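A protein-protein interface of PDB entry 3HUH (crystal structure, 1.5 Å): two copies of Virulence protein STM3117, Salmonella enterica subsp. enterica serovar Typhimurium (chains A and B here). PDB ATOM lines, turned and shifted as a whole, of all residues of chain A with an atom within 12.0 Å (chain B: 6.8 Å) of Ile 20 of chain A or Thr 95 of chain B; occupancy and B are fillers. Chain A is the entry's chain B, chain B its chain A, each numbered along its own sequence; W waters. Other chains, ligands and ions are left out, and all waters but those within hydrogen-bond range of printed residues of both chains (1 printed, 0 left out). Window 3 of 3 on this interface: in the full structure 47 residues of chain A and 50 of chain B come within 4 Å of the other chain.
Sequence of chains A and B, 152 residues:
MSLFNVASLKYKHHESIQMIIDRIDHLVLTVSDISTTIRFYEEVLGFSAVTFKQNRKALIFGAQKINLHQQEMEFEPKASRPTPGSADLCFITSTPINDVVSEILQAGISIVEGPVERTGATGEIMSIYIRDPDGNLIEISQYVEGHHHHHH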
ATOM      1  N   ILE A  20     -18.633  26.149   6.846  1.00  0.00           N
ATOM      2  CA  ILE A  20     -18.324  24.793   7.385  1.00  0.00           C
ATOM      3  C   ILE A  20     -18.717  24.699   8.855  1.00  0.00           C
ATOM      4  O   ILE A  20     -18.128  25.369   9.704  1.00  0.00           O
ATOM      5  CB  ILE A  20     -16.818  24.476   7.278  1.00  0.00           C
ATOM      6  CG1 ILE A  20     -16.372  24.507   5.810  1.00  0.00           C
ATOM      7  CG2 ILE A  20     -16.529  23.126   7.923  1.00  0.00           C
ATOM      8  CD1 ILE A  20     -17.080  23.498   4.932  1.00  0.00           C
ATOM      9  N   ILE A  21     -19.710  23.863   9.148  1.00  0.00           N
ATOM     10  CA  ILE A  21     -20.177  23.669  10.522  1.00  0.00           C
ATOM     11  C   ILE A  21     -19.488  22.436  11.102  1.00  0.00           C
ATOM     12  O   ILE A  21     -19.547  21.351  10.518  1.00  0.00           O
ATOM     13  CB  ILE A  21     -21.700  23.456  10.579  1.00  0.00           C
ATOM     14  CG1 ILE A  21     -22.431  24.698  10.054  1.00  0.00           C
ATOM     15  CG2 ILE A  21     -22.122  23.137  12.010  1.00  0.00           C
ATOM     16  CD1 ILE A  21     -22.175  25.965  10.853  1.00  0.00           C
ATOM     17  N   ASP A  22     -18.858  22.603  12.261  1.00  0.00           N
ATOM     18  CA  ASP A  22     -18.119  21.521  12.895  1.00  0.00           C
ATOM     19  C   ASP A  22     -18.884  20.681  13.912  1.00  0.00           C
ATOM     20  O   ASP A  22     -18.728  19.459  13.958  1.00  0.00           O
ATOM     21  CB  ASP A  22     -16.870  22.096  13.573  1.00  0.00           C
ATOM     22  CG  ASP A  22     -15.990  21.023  14.187  1.00  0.00           C
ATOM     23  OD1 ASP A  22     -15.311  20.301  13.425  1.00  0.00           O
ATOM     24  OD2 ASP A  22     -15.982  20.896  15.431  1.00  0.00           O
ATOM     25  N   ARG A  23     -19.717  21.331  14.715  1.00  0.00           N
ATOM     26  CA  ARG A  23     -20.435  20.626  15.766  1.00  0.00           C
ATOM     27  C   ARG A  23     -21.456  21.539  16.429  1.00  0.00           C
ATOM     28  O   ARG A  23     -21.512  22.738  16.155  1.00  0.00           O
ATOM     29  CB  ARG A  23     -19.433  20.195  16.840  1.00  0.00           C
ATOM     30  CG  ARG A  23     -18.724  21.404  17.489  1.00  0.00           C
ATOM     31  CD  ARG A  23     -17.633  20.998  18.485  1.00  0.00           C
ATOM     32  NE  ARG A  23     -17.007  22.160  19.128  1.00  0.00           N
ATOM     33  CZ  ARG A  23     -16.098  22.952  18.560  1.00  0.00           C
ATOM     34  NH1 ARG A  23     -15.679  22.727  17.322  1.00  0.00           N
ATOM     35  NH2 ARG A  23     -15.613  23.990  19.234  1.00  0.00           N
ATOM     36  N   ILE A  24     -22.256  20.953  17.314  1.00  0.00           N
ATOM     37  CA  ILE A  24     -23.233  21.701  18.093  1.00  0.00           C
ATOM     38  C   ILE A  24     -22.445  22.135  19.325  1.00  0.00           C
ATOM     39  O   ILE A  24     -21.688  21.342  19.885  1.00  0.00           O
ATOM     40  CB  ILE A  24     -24.395  20.803  18.564  1.00  0.00           C
ATOM     41  CG1 ILE A  24     -25.200  20.315  17.361  1.00  0.00           C
ATOM     42  CG2 ILE A  24     -25.282  21.565  19.543  1.00  0.00           C
ATOM     43  CD1 ILE A  24     -26.182  19.188  17.698  1.00  0.00           C
ATOM     44  N   ASP A  25     -22.591  23.389  19.731  1.00  0.00           N
ATOM     45  CA  ASP A  25     -21.892  23.873  20.911  1.00  0.00           C
ATOM     46  C   ASP A  25     -22.831  23.775  22.094  1.00  0.00           C
ATOM     47  O   ASP A  25     -22.466  23.300  23.171  1.00  0.00           O
ATOM     48  CB  ASP A  25     -21.475  25.330  20.739  1.00  0.00           C
ATOM     49  CG  ASP A  25     -20.657  25.830  21.910  1.00  0.00           C
ATOM     50  OD1 ASP A  25     -19.470  25.463  21.993  1.00  0.00           O
ATOM     51  OD2 ASP A  25     -21.202  26.573  22.759  1.00  0.00           O
ATOM     52  N   LEU B  45     -26.620  26.051   5.685  1.00  0.00           N
ATOM     53  CA  LEU B  45     -25.641  25.518   6.631  1.00  0.00           C
ATOM     54  C   LEU B  45     -24.668  24.500   6.048  1.00  0.00           C
ATOM     55  O   LEU B  45     -23.703  24.120   6.705  1.00  0.00           O
ATOM     56  CB  LEU B  45     -26.353  24.893   7.838  1.00  0.00           C
ATOM     57  CG  LEU B  45     -26.995  25.823   8.876  1.00  0.00           C
ATOM     58  CD1 LEU B  45     -25.931  26.732   9.463  1.00  0.00           C
ATOM     59  CD2 LEU B  45     -28.100  26.645   8.248  1.00  0.00           C
ATOM     60  N   GLY B  46     -24.921  24.044   4.828  1.00  0.00           N
ATOM     61  CA  GLY B  46     -24.022  23.079   4.218  1.00  0.00           C
ATOM     62  C   GLY B  46     -24.127  21.656   4.727  1.00  0.00           C
ATOM     63  O   GLY B  46     -23.202  20.860   4.543  1.00  0.00           O
ATOM     64  N   ILE B  92     -21.073  25.468  15.810  1.00  0.00           N
ATOM     65  CA  ILE B  92     -19.765  26.100  15.699  1.00  0.00           C
ATOM     66  C   ILE B  92     -19.269  25.972  14.271  1.00  0.00           C
ATOM     67  O   ILE B  92     -19.354  24.900  13.657  1.00  0.00           O
ATOM     68  CB  ILE B  92     -18.711  25.442  16.618  1.00  0.00           C
ATOM     69  CG1 ILE B  92     -19.140  25.563  18.080  1.00  0.00           C
ATOM     70  CG2 ILE B  92     -17.346  26.095  16.390  1.00  0.00           C
ATOM     71  CD1 ILE B  92     -19.373  26.988  18.550  1.00  0.00           C
ATOM     72  N   THR B  93     -18.752  27.073  13.742  1.00  0.00           N
ATOM     73  CA  THR B  93     -18.216  27.085  12.392  1.00  0.00           C
ATOM     74  C   THR B  93     -16.718  27.364  12.453  1.00  0.00           C
ATOM     75  O   THR B  93     -16.241  28.007  13.388  1.00  0.00           O
ATOM     76  CB  THR B  93     -18.877  28.173  11.520  1.00  0.00           C
ATOM     77  OG1 THR B  93     -18.340  28.107  10.192  1.00  0.00           O
ATOM     78  CG2 THR B  93     -18.605  29.562  12.089  1.00  0.00           C
ATOM     79  N   SER B  94     -15.987  26.862  11.459  1.00  0.00           N
ATOM     80  CA  SER B  94     -14.548  27.079  11.371  1.00  0.00           C
ATOM     81  C   SER B  94     -14.298  28.171  10.329  1.00  0.00           C
ATOM     82  O   SER B  94     -13.161  28.581  10.084  1.00  0.00           O
ATOM     83  CB  SER B  94     -13.828  25.782  10.972  1.00  0.00           C
ATOM     84  OG  SER B  94     -14.400  25.197   9.817  1.00  0.00           O
ATOM     85  N   THR B  95     -15.383  28.636   9.721  1.00  0.00           N
ATOM     86  CA  THR B  95     -15.322  29.691   8.716  1.00  0.00           C
ATOM     87  C   THR B  95     -15.292  31.031   9.455  1.00  0.00           C
ATOM     88  O   THR B  95     -15.991  31.203  10.453  1.00  0.00           O
ATOM     89  CB  THR B  95     -16.573  29.631   7.809  1.00  0.00           C
ATOM     90  OG1 THR B  95     -16.617  28.361   7.143  1.00  0.00           O
ATOM     91  CG2 THR B  95     -16.554  30.746   6.770  1.00  0.00           C
ATOM     92  N   PRO B  96     -14.464  31.991   8.995  1.00  0.00           N
ATOM     93  CA  PRO B  96     -14.424  33.289   9.686  1.00  0.00           C
ATOM     94  C   PRO B  96     -15.858  33.808   9.817  1.00  0.00           C
ATOM     95  O   PRO B  96     -16.589  33.871   8.828  1.00  0.00           O
ATOM     96  CB  PRO B  96     -13.571  34.146   8.756  1.00  0.00           C
ATOM     97  CG  PRO B  96     -12.623  33.141   8.156  1.00  0.00           C
ATOM     98  CD  PRO B  96     -13.545  31.978   7.842  1.00  0.00           C
ATOM     99  N   ILE B  97     -16.253  34.189  11.027  1.00  0.00           N
ATOM    100  CA  ILE B  97     -17.620  34.639  11.261  1.00  0.00           C
ATOM    101  C   ILE B  97     -18.099  35.771  10.350  1.00  0.00           C
ATOM    102  O   ILE B  97     -19.266  35.797   9.979  1.00  0.00           O
ATOM    103  CB  ILE B  97     -17.840  35.014  12.756  1.00  0.00           C
ATOM    104  CG1 ILE B  97     -19.338  34.972  13.089  1.00  0.00           C
ATOM    105  CG2 ILE B  97     -17.258  36.381  13.059  1.00  0.00           C
ATOM    106  CD1 ILE B  97     -19.965  33.588  12.912  1.00  0.00           C
ATOM    107  N   ASN B  98     -17.217  36.695   9.976  1.00  0.00           N
ATOM    108  CA  ASN B  98     -17.633  37.776   9.086  1.00  0.00           C
ATOM    109  C   ASN B  98     -17.912  37.247   7.678  1.00  0.00           C
ATOM    110  O   ASN B  98     -18.764  37.784   6.957  1.00  0.00           O
ATOM    111  CB  ASN B  98     -16.578  38.889   9.053  1.00  0.00           C
ATOM    112  CG  ASN B  98     -16.538  39.683  10.350  1.00  0.00           C
ATOM    113  OD1 ASN B  98     -17.414  39.530  11.208  1.00  0.00           O
ATOM    114  ND2 ASN B  98     -15.533  40.540  10.497  1.00  0.00           N
ATOM    115  N   ASP B  99     -17.207  36.194   7.277  1.00  0.00           N
ATOM    116  CA  ASP B  99     -17.454  35.610   5.966  1.00  0.00           C
ATOM    117  C   ASP B  99     -18.818  34.922   6.027  1.00  0.00           C
ATOM    118  O   ASP B  99     -19.576  34.925   5.053  1.00  0.00           O
ATOM    119  CB  ASP B  99     -16.370  34.584   5.594  1.00  0.00           C
ATOM    120  CG  ASP B  99     -15.025  35.230   5.289  1.00  0.00           C
ATOM    121  OD1 ASP B  99     -14.989  36.429   4.928  1.00  0.00           O
ATOM    122  OD2 ASP B  99     -13.998  34.527   5.392  1.00  0.00           O
ATOM    123  N   VAL B 100     -19.138  34.345   7.186  1.00  0.00           N
ATOM    124  CA  VAL B 100     -20.421  33.674   7.357  1.00  0.00           C
ATOM    125  C   VAL B 100     -21.539  34.708   7.268  1.00  0.00           C
ATOM    126  O   VAL B 100     -22.568  34.468   6.637  1.00  0.00           O
ATOM    127  CB  VAL B 100     -20.515  32.962   8.727  1.00  0.00           C
ATOM    128  CG1 VAL B 100     -21.908  32.361   8.908  1.00  0.00           C
ATOM    129  CG2 VAL B 100     -19.454  31.867   8.819  1.00  0.00           C
ATOM    130  N   GLU B 103     -22.107  35.438   3.766  1.00  0.00           N
ATOM    131  CA  GLU B 103     -22.724  34.286   3.120  1.00  0.00           C
ATOM    132  C   GLU B 103     -24.234  34.283   3.361  1.00  0.00           C
ATOM    133  O   GLU B 103     -25.022  34.041   2.443  1.00  0.00           O
ATOM    134  CB  GLU B 103     -22.093  33.008   3.677  1.00  0.00           C
ATOM    135  CG  GLU B 103     -22.299  31.757   2.858  1.00  0.00           C
ATOM    136  CD  GLU B 103     -21.503  30.589   3.417  1.00  0.00           C
ATOM    137  OE1 GLU B 103     -20.280  30.748   3.618  1.00  0.00           O
ATOM    138  OE2 GLU B 103     -22.095  29.519   3.655  1.00  0.00           O
ATOM    139  N   ILE B 140     -25.138  30.611  14.763  1.00  0.00           N
ATOM    140  CA  ILE B 140     -23.921  30.123  14.111  1.00  0.00           C
ATOM    141  C   ILE B 140     -22.778  30.909  14.743  1.00  0.00           C
ATOM    142  O   ILE B 140     -22.759  32.145  14.692  1.00  0.00           O
ATOM    143  CB  ILE B 140     -23.968  30.346  12.590  1.00  0.00           C
ATOM    144  CG1 ILE B 140     -25.182  29.618  12.007  1.00  0.00           C
ATOM    145  CG2 ILE B 140     -22.704  29.803  11.949  1.00  0.00           C
ATOM    146  CD1 ILE B 140     -25.507  29.976  10.577  1.00  0.00           C
ATOM    147  N   SER B 141     -21.821  30.196  15.328  1.00  0.00           N
ATOM    148  CA  SER B 141     -20.741  30.865  16.044  1.00  0.00           C
ATOM    149  C   SER B 141     -19.320  30.375  15.798  1.00  0.00           C
ATOM    150  O   SER B 141     -19.092  29.225  15.445  1.00  0.00           O
ATOM    151  CB  SER B 141     -21.031  30.768  17.545  1.00  0.00           C
ATOM    152  OG  SER B 141     -22.409  30.984  17.808  1.00  0.00           O
ATOM    153  N   GLN B 142     -18.363  31.275  16.002  1.00  0.00           N
ATOM    154  CA  GLN B 142     -16.952  30.948  15.862  1.00  0.00           C
ATOM    155  C   GLN B 142     -16.283  31.303  17.183  1.00  0.00           C
ATOM    156  O   GLN B 142     -16.540  32.373  17.746  1.00  0.00           O
ATOM    157  CB  GLN B 142     -16.307  31.759  14.734  1.00  0.00           C
ATOM    158  CG  GLN B 142     -14.796  31.593  14.664  1.00  0.00           C
ATOM    159  CD  GLN B 142     -14.167  32.432  13.575  1.00  0.00           C
ATOM    160  OE1 GLN B 142     -14.565  33.574  13.347  1.00  0.00           O
ATOM    161  NE2 GLN B 142     -13.166  31.874  12.903  1.00  0.00           N
HETATM  162  O   HOH W   1     -21.305  22.812   7.063  1.00  0.00           O
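Water W1 lies within hydrogen-bond range of O of Leu 45 of chain B (2.8 Å) and N of Ile 21 of chain A (2.8 Å).
The backbone carbonyl oxygen (O) of Ile 92 of chain B lies within hydrogen-bond range of the backbone NH (N) of Asp 22 of chain A (2.7 Å).
O of Arg 23 of chain A sits at hydrogen-bond distance from N of Ile 92 of chain B (2.8 Å).
The backbone carbonyl oxygen of Ile 20 of chain A is in hydrogen-bond range of the side-chain hydroxyl of Thr 93 of chain B.
O of Ile 20 of chain A lies within hydrogen-bond range of N of Ser 94 of chain B.
The backbone NH (N) of Ile 20 of chain A sits at hydrogen-bond distance from the side-chain hydroxyl (OG1) of Thr 95 of chain B, 3.0 Å away.
Of chain B, only Thr 93 (2.8 Å), Ser 94 (3.1 Å) and Thr 95 (3.0 Å) come within 4 Å of Ile 20 of chain A.
Printed residues of chain B within 4 Å of Ile 21 of chain A: Leu 45 (3.6 Å) and Ile 92 (3.5 Å).
Printed residues of chain B within 4 Å of Arg 23 of chain A: Ile 92 (2.8 Å).
Printed residues of chain B within 4 Å of Asp 25 of chain A: Ile 92 (3.5 Å).
No residue of chain A comes within 4 Å of Gly 46 of chain B.
Printed residues of chain A within 4 Å of Ile 92 of chain B: Ile 21, Asp 22, Arg 23 and Asp 25.
Of the printed residues of chain A, Thr 93 of chain B touches Ile 20 (2.8 Å).
Ser 94 of chain B touches one residue of chain A.
No residue of chain A comes within 4 Å of Pro 96 of chain B.
Ile 97 of chain B touches none of the printed residues of chain A.
No residue of chain A comes within 4 Å of Gln 142 of chain B.
The side-chain hydroxyl (OG1) of Thr 93 of chain B is in hydrogen-bond range of the backbone NH (N) of Thr 95 of chain B, at 3.0 Å.
The backbone carbonyl oxygen of Ser 141 of chain B lies within hydrogen-bond range of the backbone NH of Thr 93 of chain B.
The guanidinium group (NH1) of Arg 23 of chain A lies within salt-bridge range of the side-chain carboxylate (OD2) of Asp 22 of chain A, at 2.6 Å.
No position is printed for both chains.
Of the 8 pairs that touch across the chains among the printed residues, none has its exchanged pair printed and touching as well.
Among the printed residues, pairs that only touch across the chains: Ile 21 of chain A with Leu 45 of chain B (3.6 Å), Ile 21 of chain A with Ile 92 of chain B (3.5 Å) and Asp 25 of chain A with Ile 92 of chain B (3.5 Å).
Of the 15 printed residues of chain B, 5 touch a printed residue of chain A.
Printed residues of chain B that touch a printed residue of chain A: Leu 45, Ile 92, Thr 93, Ser 94 and Thr 95.
Hydrophobic or aromatic side chains of chain B within 4 Å of the printed part of chain A: Ile 92.
Along chain A the printed residues that touch a printed residue of chain B span positions 20 to 25.
Among the printed residues, 8 pairs touch across the chains.
Among the printed residues, no Asp or Glu carboxylate lies within 4 Å of a Lys or Arg side-chain nitrogen of the other chain.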
